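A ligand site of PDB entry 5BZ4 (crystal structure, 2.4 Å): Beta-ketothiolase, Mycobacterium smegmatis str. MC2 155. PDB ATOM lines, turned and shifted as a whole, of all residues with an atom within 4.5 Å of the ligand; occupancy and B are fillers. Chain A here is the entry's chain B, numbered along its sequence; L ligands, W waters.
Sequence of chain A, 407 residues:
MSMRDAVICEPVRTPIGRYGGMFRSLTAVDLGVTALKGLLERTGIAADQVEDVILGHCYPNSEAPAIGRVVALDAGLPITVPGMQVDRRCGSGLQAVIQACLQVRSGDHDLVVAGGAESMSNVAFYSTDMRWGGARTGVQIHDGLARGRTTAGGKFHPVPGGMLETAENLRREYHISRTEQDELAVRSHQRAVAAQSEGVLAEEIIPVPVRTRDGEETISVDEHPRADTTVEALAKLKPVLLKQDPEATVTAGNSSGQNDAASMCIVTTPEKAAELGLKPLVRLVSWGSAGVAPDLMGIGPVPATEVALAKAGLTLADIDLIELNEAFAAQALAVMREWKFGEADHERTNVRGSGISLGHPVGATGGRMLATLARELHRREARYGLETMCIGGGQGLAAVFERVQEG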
ATOM      1  N   TYR A  19     -26.825 -10.530  -6.175  1.00  0.00           N
ATOM      2  CA  TYR A  19     -27.187 -11.867  -5.750  1.00  0.00           C
ATOM      3  C   TYR A  19     -28.241 -12.410  -6.700  1.00  0.00           C
ATOM      4  O   TYR A  19     -29.324 -11.832  -6.794  1.00  0.00           O
ATOM      5  CB  TYR A  19     -27.714 -11.816  -4.326  1.00  0.00           C
ATOM      6  CG  TYR A  19     -28.143 -13.108  -3.703  1.00  0.00           C
ATOM      7  CD1 TYR A  19     -27.261 -14.133  -3.527  1.00  0.00           C
ATOM      8  CD2 TYR A  19     -29.436 -13.280  -3.231  1.00  0.00           C
ATOM      9  CE1 TYR A  19     -27.626 -15.313  -2.943  1.00  0.00           C
ATOM     10  CE2 TYR A  19     -29.823 -14.459  -2.636  1.00  0.00           C
ATOM     11  CZ  TYR A  19     -28.907 -15.470  -2.494  1.00  0.00           C
ATOM     12  OH  TYR A  19     -29.246 -16.665  -1.903  1.00  0.00           O
ATOM     13  N   CYS A  90     -14.891 -11.813   5.743  1.00  0.00           N
ATOM     14  CA  CYS A  90     -14.792 -10.554   5.009  1.00  0.00           C
ATOM     15  C   CYS A  90     -13.364 -10.047   4.769  1.00  0.00           C
ATOM     16  O   CYS A  90     -13.080  -9.448   3.735  1.00  0.00           O
ATOM     17  CB  CYS A  90     -15.617  -9.486   5.721  1.00  0.00           C
ATOM     18  SG  CYS A  90     -17.331 -10.007   6.096  1.00  0.00           S
ATOM     19  N   ARG A 149     -22.997 -17.682   9.400  1.00  0.00           N
ATOM     20  CA  ARG A 149     -23.107 -16.393  10.105  1.00  0.00           C
ATOM     21  C   ARG A 149     -23.569 -16.541  11.550  1.00  0.00           C
ATOM     22  O   ARG A 149     -23.451 -15.612  12.340  1.00  0.00           O
ATOM     23  CB  ARG A 149     -24.037 -15.453   9.323  1.00  0.00           C
ATOM     24  CG  ARG A 149     -23.417 -14.870   8.063  1.00  0.00           C
ATOM     25  CD  ARG A 149     -24.437 -14.370   7.075  1.00  0.00           C
ATOM     26  NE  ARG A 149     -23.804 -13.921   5.845  1.00  0.00           N
ATOM     27  CZ  ARG A 149     -24.440 -13.683   4.695  1.00  0.00           C
ATOM     28  NH1 ARG A 149     -25.753 -13.839   4.601  1.00  0.00           N
ATOM     29  NH2 ARG A 149     -23.758 -13.280   3.640  1.00  0.00           N
ATOM     30  N   MET A 163     -25.380 -12.042  10.993  1.00  0.00           N
ATOM     31  CA  MET A 163     -24.725 -10.748  10.911  1.00  0.00           C
ATOM     32  C   MET A 163     -25.672  -9.601  11.206  1.00  0.00           C
ATOM     33  O   MET A 163     -25.315  -8.685  11.940  1.00  0.00           O
ATOM     34  CB  MET A 163     -24.095 -10.557   9.530  1.00  0.00           C
ATOM     35  CG  MET A 163     -23.044 -11.557   9.206  1.00  0.00           C
ATOM     36  SD  MET A 163     -21.678 -11.397  10.367  1.00  0.00           S
ATOM     37  CE  MET A 163     -21.587 -13.021  11.106  1.00  0.00           C
ATOM     38  N   LEU A 164     -26.856  -9.640  10.604  1.00  0.00           N
ATOM     39  CA  LEU A 164     -27.877  -8.625  10.844  1.00  0.00           C
ATOM     40  C   LEU A 164     -28.119  -8.471  12.329  1.00  0.00           C
ATOM     41  O   LEU A 164     -28.284  -7.366  12.805  1.00  0.00           O
ATOM     42  CB  LEU A 164     -29.177  -8.982  10.124  1.00  0.00           C
ATOM     43  CG  LEU A 164     -29.181  -9.007   8.590  1.00  0.00           C
ATOM     44  CD1 LEU A 164     -30.013 -10.172   8.088  1.00  0.00           C
ATOM     45  CD2 LEU A 164     -29.690  -7.715   8.000  1.00  0.00           C
ATOM     46  N   HIS A 189     -24.527   5.143  -2.295  1.00  0.00           N
ATOM     47  CA  HIS A 189     -24.915   4.952  -3.694  1.00  0.00           C
ATOM     48  C   HIS A 189     -24.546   6.144  -4.567  1.00  0.00           C
ATOM     49  O   HIS A 189     -24.161   5.998  -5.724  1.00  0.00           O
ATOM     50  CB  HIS A 189     -26.407   4.692  -3.791  1.00  0.00           C
ATOM     51  CG  HIS A 189     -26.800   3.302  -3.400  1.00  0.00           C
ATOM     52  ND1 HIS A 189     -26.916   2.276  -4.321  1.00  0.00           N
ATOM     53  CD2 HIS A 189     -27.093   2.760  -2.200  1.00  0.00           C
ATOM     54  CE1 HIS A 189     -27.269   1.171  -3.697  1.00  0.00           C
ATOM     55  NE2 HIS A 189     -27.387   1.432  -2.409  1.00  0.00           N
ATOM     56  N   ARG A 226     -27.492   2.119  -7.293  1.00  0.00           N
ATOM     57  CA  ARG A 226     -28.791   2.636  -7.747  1.00  0.00           C
ATOM     58  C   ARG A 226     -28.799   4.163  -7.881  1.00  0.00           C
ATOM     59  O   ARG A 226     -28.545   4.879  -6.918  1.00  0.00           O
ATOM     60  CB  ARG A 226     -29.895   2.209  -6.783  1.00  0.00           C
ATOM     61  CG  ARG A 226     -30.014   0.711  -6.621  1.00  0.00           C
ATOM     62  CD  ARG A 226     -30.499   0.309  -5.242  1.00  0.00           C
ATOM     63  NE  ARG A 226     -31.937   0.113  -5.236  1.00  0.00           N
ATOM     64  CZ  ARG A 226     -32.550  -1.071  -5.276  1.00  0.00           C
ATOM     65  NH1 ARG A 226     -31.846  -2.197  -5.318  1.00  0.00           N
ATOM     66  NH2 ARG A 226     -33.873  -1.126  -5.280  1.00  0.00           N
ATOM     67  N   THR A 229     -31.641   6.191  -5.356  1.00  0.00           N
ATOM     68  CA  THR A 229     -31.807   5.941  -3.927  1.00  0.00           C
ATOM     69  C   THR A 229     -32.191   7.216  -3.176  1.00  0.00           C
ATOM     70  O   THR A 229     -31.530   8.239  -3.339  1.00  0.00           O
ATOM     71  CB  THR A 229     -30.505   5.404  -3.309  1.00  0.00           C
ATOM     72  OG1 THR A 229     -30.087   4.237  -4.007  1.00  0.00           O
ATOM     73  CG2 THR A 229     -30.716   5.053  -1.857  1.00  0.00           C
ATOM     74  N   LEU A 234     -35.845   4.700   1.178  1.00  0.00           N
ATOM     75  CA  LEU A 234     -35.269   3.787   2.161  1.00  0.00           C
ATOM     76  C   LEU A 234     -36.157   3.623   3.378  1.00  0.00           C
ATOM     77  O   LEU A 234     -36.279   2.521   3.913  1.00  0.00           O
ATOM     78  CB  LEU A 234     -33.889   4.273   2.594  1.00  0.00           C
ATOM     79  CG  LEU A 234     -32.783   4.073   1.565  1.00  0.00           C
ATOM     80  CD1 LEU A 234     -31.432   4.408   2.143  1.00  0.00           C
ATOM     81  CD2 LEU A 234     -32.821   2.635   1.094  1.00  0.00           C
ATOM     82  N   LEU A 237     -38.663   0.639   3.824  1.00  0.00           N
ATOM     83  CA  LEU A 237     -38.278  -0.758   3.989  1.00  0.00           C
ATOM     84  C   LEU A 237     -38.451  -1.293   5.418  1.00  0.00           C
ATOM     85  O   LEU A 237     -38.217  -0.588   6.398  1.00  0.00           O
ATOM     86  CB  LEU A 237     -36.833  -0.950   3.537  1.00  0.00           C
ATOM     87  CG  LEU A 237     -36.492  -0.372   2.172  1.00  0.00           C
ATOM     88  CD1 LEU A 237     -35.014  -0.568   1.836  1.00  0.00           C
ATOM     89  CD2 LEU A 237     -37.395  -0.971   1.087  1.00  0.00           C
ATOM     90  N   VAL A 240     -34.962  -6.433   8.651  1.00  0.00           N
ATOM     91  CA  VAL A 240     -35.049  -7.868   8.450  1.00  0.00           C
ATOM     92  C   VAL A 240     -35.540  -8.537   9.729  1.00  0.00           C
ATOM     93  O   VAL A 240     -36.280  -9.520   9.679  1.00  0.00           O
ATOM     94  CB  VAL A 240     -33.692  -8.460   8.019  1.00  0.00           C
ATOM     95  CG1 VAL A 240     -33.781  -9.972   7.928  1.00  0.00           C
ATOM     96  CG2 VAL A 240     -33.262  -7.909   6.678  1.00  0.00           C
ATOM     97  N   THR A 251     -31.919  -3.011   7.369  1.00  0.00           N
ATOM     98  CA  THR A 251     -32.720  -3.463   6.239  1.00  0.00           C
ATOM     99  C   THR A 251     -31.868  -3.937   5.071  1.00  0.00           C
ATOM    100  O   THR A 251     -30.635  -3.908   5.141  1.00  0.00           O
ATOM    101  CB  THR A 251     -33.631  -2.340   5.714  1.00  0.00           C
ATOM    102  OG1 THR A 251     -32.827  -1.311   5.126  1.00  0.00           O
ATOM    103  CG2 THR A 251     -34.445  -1.740   6.834  1.00  0.00           C
ATOM    104  N   ALA A 252     -32.526  -4.342   4.004  1.00  0.00           N
ATOM    105  CA  ALA A 252     -31.846  -4.603   2.750  1.00  0.00           C
ATOM    106  C   ALA A 252     -31.116  -3.343   2.267  1.00  0.00           C
ATOM    107  O   ALA A 252     -29.975  -3.406   1.806  1.00  0.00           O
ATOM    108  CB  ALA A 252     -32.825  -5.065   1.705  1.00  0.00           C
ATOM    109  N   GLY A 253     -31.785  -2.199   2.405  1.00  0.00           N
ATOM    110  CA  GLY A 253     -31.287  -0.920   1.920  1.00  0.00           C
ATOM    111  C   GLY A 253     -30.071  -0.386   2.663  1.00  0.00           C
ATOM    112  O   GLY A 253     -29.208   0.215   2.043  1.00  0.00           O
ATOM    113  N   SER A 255     -27.957  -2.396   4.412  1.00  0.00           N
ATOM    114  CA  SER A 255     -26.998  -3.478   4.590  1.00  0.00           C
ATOM    115  C   SER A 255     -26.198  -3.624   3.315  1.00  0.00           C
ATOM    116  O   SER A 255     -26.663  -3.204   2.255  1.00  0.00           O
ATOM    117  CB  SER A 255     -27.695  -4.798   4.909  1.00  0.00           C
ATOM    118  OG  SER A 255     -28.629  -4.651   5.944  1.00  0.00           O
ATOM    119  N   SER A 256     -25.012  -4.203   3.417  1.00  0.00           N
ATOM    120  CA  SER A 256     -24.261  -4.584   2.233  1.00  0.00           C
ATOM    121  C   SER A 256     -25.028  -5.678   1.515  1.00  0.00           C
ATOM    122  O   SER A 256     -25.879  -6.345   2.105  1.00  0.00           O
ATOM    123  CB  SER A 256     -22.854  -5.052   2.598  1.00  0.00           C
ATOM    124  OG  SER A 256     -22.861  -6.285   3.301  1.00  0.00           O
ATOM    125  N   GLY A 257     -24.775  -5.833   0.216  1.00  0.00           N
ATOM    126  CA  GLY A 257     -25.442  -6.869  -0.539  1.00  0.00           C
ATOM    127  C   GLY A 257     -24.642  -8.154  -0.556  1.00  0.00           C
ATOM    128  O   GLY A 257     -23.490  -8.206  -0.143  1.00  0.00           O
ATOM    129  N   GLN A 258     -25.275  -9.214  -1.045  1.00  0.00           N
ATOM    130  CA  GLN A 258     -24.589 -10.453  -1.331  1.00  0.00           C
ATOM    131  C   GLN A 258     -24.316 -10.487  -2.841  1.00  0.00           C
ATOM    132  O   GLN A 258     -25.212 -10.202  -3.625  1.00  0.00           O
ATOM    133  CB  GLN A 258     -25.419 -11.632  -0.837  1.00  0.00           C
ATOM    134  CG  GLN A 258     -25.703 -11.477   0.648  1.00  0.00           C
ATOM    135  CD  GLN A 258     -26.475 -12.606   1.229  1.00  0.00           C
ATOM    136  OE1 GLN A 258     -25.951 -13.357   2.055  1.00  0.00           O
ATOM    137  NE2 GLN A 258     -27.736 -12.721   0.839  1.00  0.00           N
ATOM    138  N   MET A 297     -18.851  -8.179  16.391  1.00  0.00           N
ATOM    139  CA  MET A 297     -17.800  -8.264  15.411  1.00  0.00           C
ATOM    140  C   MET A 297     -17.638  -6.924  14.707  1.00  0.00           C
ATOM    141  O   MET A 297     -16.529  -6.562  14.330  1.00  0.00           O
ATOM    142  CB  MET A 297     -18.132  -9.308  14.364  1.00  0.00           C
ATOM    143  CG  MET A 297     -18.708  -8.513  13.292  1.00  0.00           C
ATOM    144  SD  MET A 297     -19.142  -8.776  11.700  1.00  0.00           S
ATOM    145  CE  MET A 297     -20.753  -9.245  12.305  1.00  0.00           C
ATOM    146  N   ALA A 327     -20.278  -3.105   5.922  1.00  0.00           N
ATOM    147  CA  ALA A 327     -20.992  -4.363   6.090  1.00  0.00           C
ATOM    148  C   ALA A 327     -22.437  -4.037   6.387  1.00  0.00           C
ATOM    149  O   ALA A 327     -23.354  -4.566   5.758  1.00  0.00           O
ATOM    150  CB  ALA A 327     -20.402  -5.200   7.186  1.00  0.00           C
ATOM    151  N   PHE A 328     -22.628  -3.142   7.365  1.00  0.00           N
ATOM    152  CA  PHE A 328     -23.936  -2.561   7.648  1.00  0.00           C
ATOM    153  C   PHE A 328     -23.742  -1.090   7.990  1.00  0.00           C
ATOM    154  O   PHE A 328     -22.777  -0.749   8.651  1.00  0.00           O
ATOM    155  CB  PHE A 328     -24.641  -3.295   8.783  1.00  0.00           C
ATOM    156  CG  PHE A 328     -24.825  -4.757   8.526  1.00  0.00           C
ATOM    157  CD1 PHE A 328     -25.897  -5.213   7.775  1.00  0.00           C
ATOM    158  CD2 PHE A 328     -23.923  -5.679   9.047  1.00  0.00           C
ATOM    159  CE1 PHE A 328     -26.068  -6.544   7.527  1.00  0.00           C
ATOM    160  CE2 PHE A 328     -24.085  -7.026   8.811  1.00  0.00           C
ATOM    161  CZ  PHE A 328     -25.149  -7.464   8.045  1.00  0.00           C
ATOM    162  N   HIS A 360     -20.972  -6.597  -1.795  1.00  0.00           N
ATOM    163  CA  HIS A 360     -19.986  -7.209  -0.919  1.00  0.00           C
ATOM    164  C   HIS A 360     -19.740  -8.669  -1.274  1.00  0.00           C
ATOM    165  O   HIS A 360     -20.125  -9.566  -0.526  1.00  0.00           O
ATOM    166  CB  HIS A 360     -20.445  -7.069   0.535  1.00  0.00           C
ATOM    167  CG  HIS A 360     -19.447  -7.532   1.545  1.00  0.00           C
ATOM    168  ND1 HIS A 360     -18.129  -7.762   1.252  1.00  0.00           N
ATOM    169  CD2 HIS A 360     -19.592  -7.787   2.868  1.00  0.00           C
ATOM    170  CE1 HIS A 360     -17.495  -8.151   2.346  1.00  0.00           C
ATOM    171  NE2 HIS A 360     -18.355  -8.175   3.338  1.00  0.00           N
HETATM  172  N1  LIG L   1     -33.435   1.562  -1.924  1.00  0.00           N
HETATM  173  C1  LIG L   1     -34.732   1.130  -2.043  1.00  0.00           C
HETATM  174  N2  LIG L   1     -35.042  -0.214  -1.969  1.00  0.00           N
HETATM  175  C2  LIG L   1     -34.035  -1.137  -1.772  1.00  0.00           C
HETATM  176  C3  LIG L   1     -32.751  -0.709  -1.657  1.00  0.00           C
HETATM  177  C4  LIG L   1     -32.443   0.647  -1.738  1.00  0.00           C
HETATM  178  N3  LIG L   1     -31.153   1.291  -1.636  1.00  0.00           N
HETATM  179  N4  LIG L   1     -31.964  -1.818  -1.469  1.00  0.00           N
HETATM  180  C5  LIG L   1     -32.734  -2.898  -1.477  1.00  0.00           C
HETATM  181  N5  LIG L   1     -34.031  -2.477  -1.657  1.00  0.00           N
HETATM  182  C6  LIG L   1     -35.215  -3.240  -1.754  1.00  0.00           C
HETATM  183  C7  LIG L   1     -35.110  -4.005  -2.813  1.00  0.00           C
HETATM  184  O1  LIG L   1     -35.539  -3.358  -4.028  1.00  0.00           O
HETATM  185  C8  LIG L   1     -36.021  -5.340  -2.511  1.00  0.00           C
HETATM  186  O2  LIG L   1     -37.365  -5.047  -2.851  1.00  0.00           O
HETATM  187  P1  LIG L   1     -38.226  -6.014  -3.809  1.00  0.00           P
HETATM  188  O3  LIG L   1     -39.548  -5.336  -4.021  1.00  0.00           O
HETATM  189  O4  LIG L   1     -38.371  -7.375  -3.124  1.00  0.00           O
HETATM  190  O5  LIG L   1     -37.520  -6.178  -5.154  1.00  0.00           O
HETATM  191  C9  LIG L   1     -35.888  -5.559  -1.167  1.00  0.00           C
HETATM  192  O6  LIG L   1     -35.325  -4.292  -0.538  1.00  0.00           O
HETATM  193  C10 LIG L   1     -34.954  -6.737  -0.861  1.00  0.00           C
HETATM  194  O7  LIG L   1     -33.656  -6.533  -1.353  1.00  0.00           O
HETATM  195  P2  LIG L   1     -32.938  -7.724  -2.068  1.00  0.00           P
HETATM  196  O8  LIG L   1     -33.961  -8.521  -2.864  1.00  0.00           O
HETATM  197  O9  LIG L   1     -31.873  -7.204  -3.038  1.00  0.00           O
HETATM  198  O10 LIG L   1     -32.205  -8.656  -0.980  1.00  0.00           O
HETATM  199  P3  LIG L   1     -32.764  -9.900  -0.146  1.00  0.00           P
HETATM  200  O11 LIG L   1     -34.257  -9.866  -0.095  1.00  0.00           O
HETATM  201  O12 LIG L   1     -32.264 -11.181  -0.747  1.00  0.00           O
HETATM  202  O13 LIG L   1     -32.223  -9.783   1.340  1.00  0.00           O
HETATM  203  C11 LIG L   1     -30.398  -9.101   2.916  1.00  0.00           C
HETATM  204  C12 LIG L   1     -31.287  -8.743   1.645  1.00  0.00           C
HETATM  205  C13 LIG L   1     -31.138 -10.121   3.846  1.00  0.00           C
HETATM  206  C14 LIG L   1     -30.022  -7.825   3.690  1.00  0.00           C
HETATM  207  C15 LIG L   1     -29.049  -9.749   2.380  1.00  0.00           C
HETATM  208  O14 LIG L   1     -28.550  -9.008   1.345  1.00  0.00           O
HETATM  209  C16 LIG L   1     -27.976  -9.771   3.396  1.00  0.00           C
HETATM  210  O15 LIG L   1     -27.884 -10.676   4.194  1.00  0.00           O
HETATM  211  N6  LIG L   1     -27.013  -8.734   3.371  1.00  0.00           N
HETATM  212  C17 LIG L   1     -25.948  -8.753   4.309  1.00  0.00           C
HETATM  213  C18 LIG L   1     -24.843  -9.587   3.669  1.00  0.00           C
HETATM  214  C19 LIG L   1     -23.760  -9.914   4.702  1.00  0.00           C
HETATM  215  O16 LIG L   1     -24.046 -10.371   5.827  1.00  0.00           O
HETATM  216  N7  LIG L   1     -22.415  -9.677   4.319  1.00  0.00           N
HETATM  217  C20 LIG L   1     -21.382  -9.966   5.263  1.00  0.00           C
HETATM  218  C21 LIG L   1     -21.144  -8.699   6.179  1.00  0.00           C
HETATM  219  S1  LIG L   1     -20.332  -9.189   7.693  1.00  0.00           S
HETATM  220  O   HOH W   1     -22.062 -10.121   1.589  1.00  0.00           O
HETATM  221  O   HOH W   2     -20.876 -13.331   5.027  1.00  0.00           O
HETATM  222  O   HOH W   3     -28.871  -0.121  -0.877  1.00  0.00           O
HETATM  223  O   HOH W   4     -29.153  -6.028   0.838  1.00  0.00           O
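N6 of the ligand is in hydrogen-bond range of O of Ser 256 (2.9 Å).
NH2 of Arg 226 is in hydrogen-bond range of O1 of the ligand (3.1 Å).
The side-chain sulfur (SG) of Cys 90 sits close to a sulfur (S1) of the ligand (3.5 Å).
A sulfur (S1) of the ligand lies close to the side-chain sulfur (SD) of Met 163 (3.7 Å).
Water W3 lies within hydrogen-bond range of NE2 of His 189, N3 of the ligand and O of Gly 253.
Water W1 lies within hydrogen-bond range of a nitrogen (N7) of the ligand, the backbone carbonyl oxygen of His 360 and the backbone carbonyl oxygen of Gly 257.
Water W4 lies within hydrogen-bond range of the backbone carbonyl oxygen of Ala 252 and an oxygen (O14) of the ligand.
Arg 149 touches the ligand (CZ to O16, 3.5 Å).
His 189 touches the ligand.
CG2 of Thr 229 touches N3 of the ligand (3.8 Å).
Leu 234 touches the ligand (CD2 to N1, 3.3 Å).
Leu 237 touches the ligand (CD1 to C2, 3.8 Å).
CB of Ala 252 touches O6 of the ligand (3.4 Å).
Gly 253 touches the ligand.
Gln 258 touches the ligand.
Ala 327 touches the ligand.
CZ of Phe 328 touches O16 of the ligand, 3.8 Å away.
His 360 touches the ligand.
Hydrophobic or aromatic side chains within 4 Å of the ligand: Met 163, Leu 234, Leu 237, Ala 252, Ala 327, Phe 328 and His 360.
The nearest printed residue that does not touch the ligand is Ser 255 (4.01 Å).
O of Ala 327 lies within hydrogen-bond range of N of Ser 256, 2.9 Å away.
The side-chain hydroxyl of Thr 229 is in hydrogen-bond range of the backbone carbonyl oxygen of Arg 226.
N of Arg 226 lies within hydrogen-bond range of ND1 of His 189, at 3.0 Å.
NE2 of His 360 sits at hydrogen-bond distance from SG of Cys 90 (3.5 Å).
The guanidinium group (NH1) of Arg 149 sits at hydrogen-bond distance from the side-chain amide oxygen (OE1) of Gln 258, 2.6 Å away.
N of Gly 253 lies within hydrogen-bond range of OG1 of Thr 251 (3.0 Å).
The backbone NH (N) of Tyr 19 is in hydrogen-bond range of the backbone carbonyl oxygen (O) of Gln 258, 3.0 Å away.
N of His 360 sits close to O of Gly 257 (3.4 Å).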
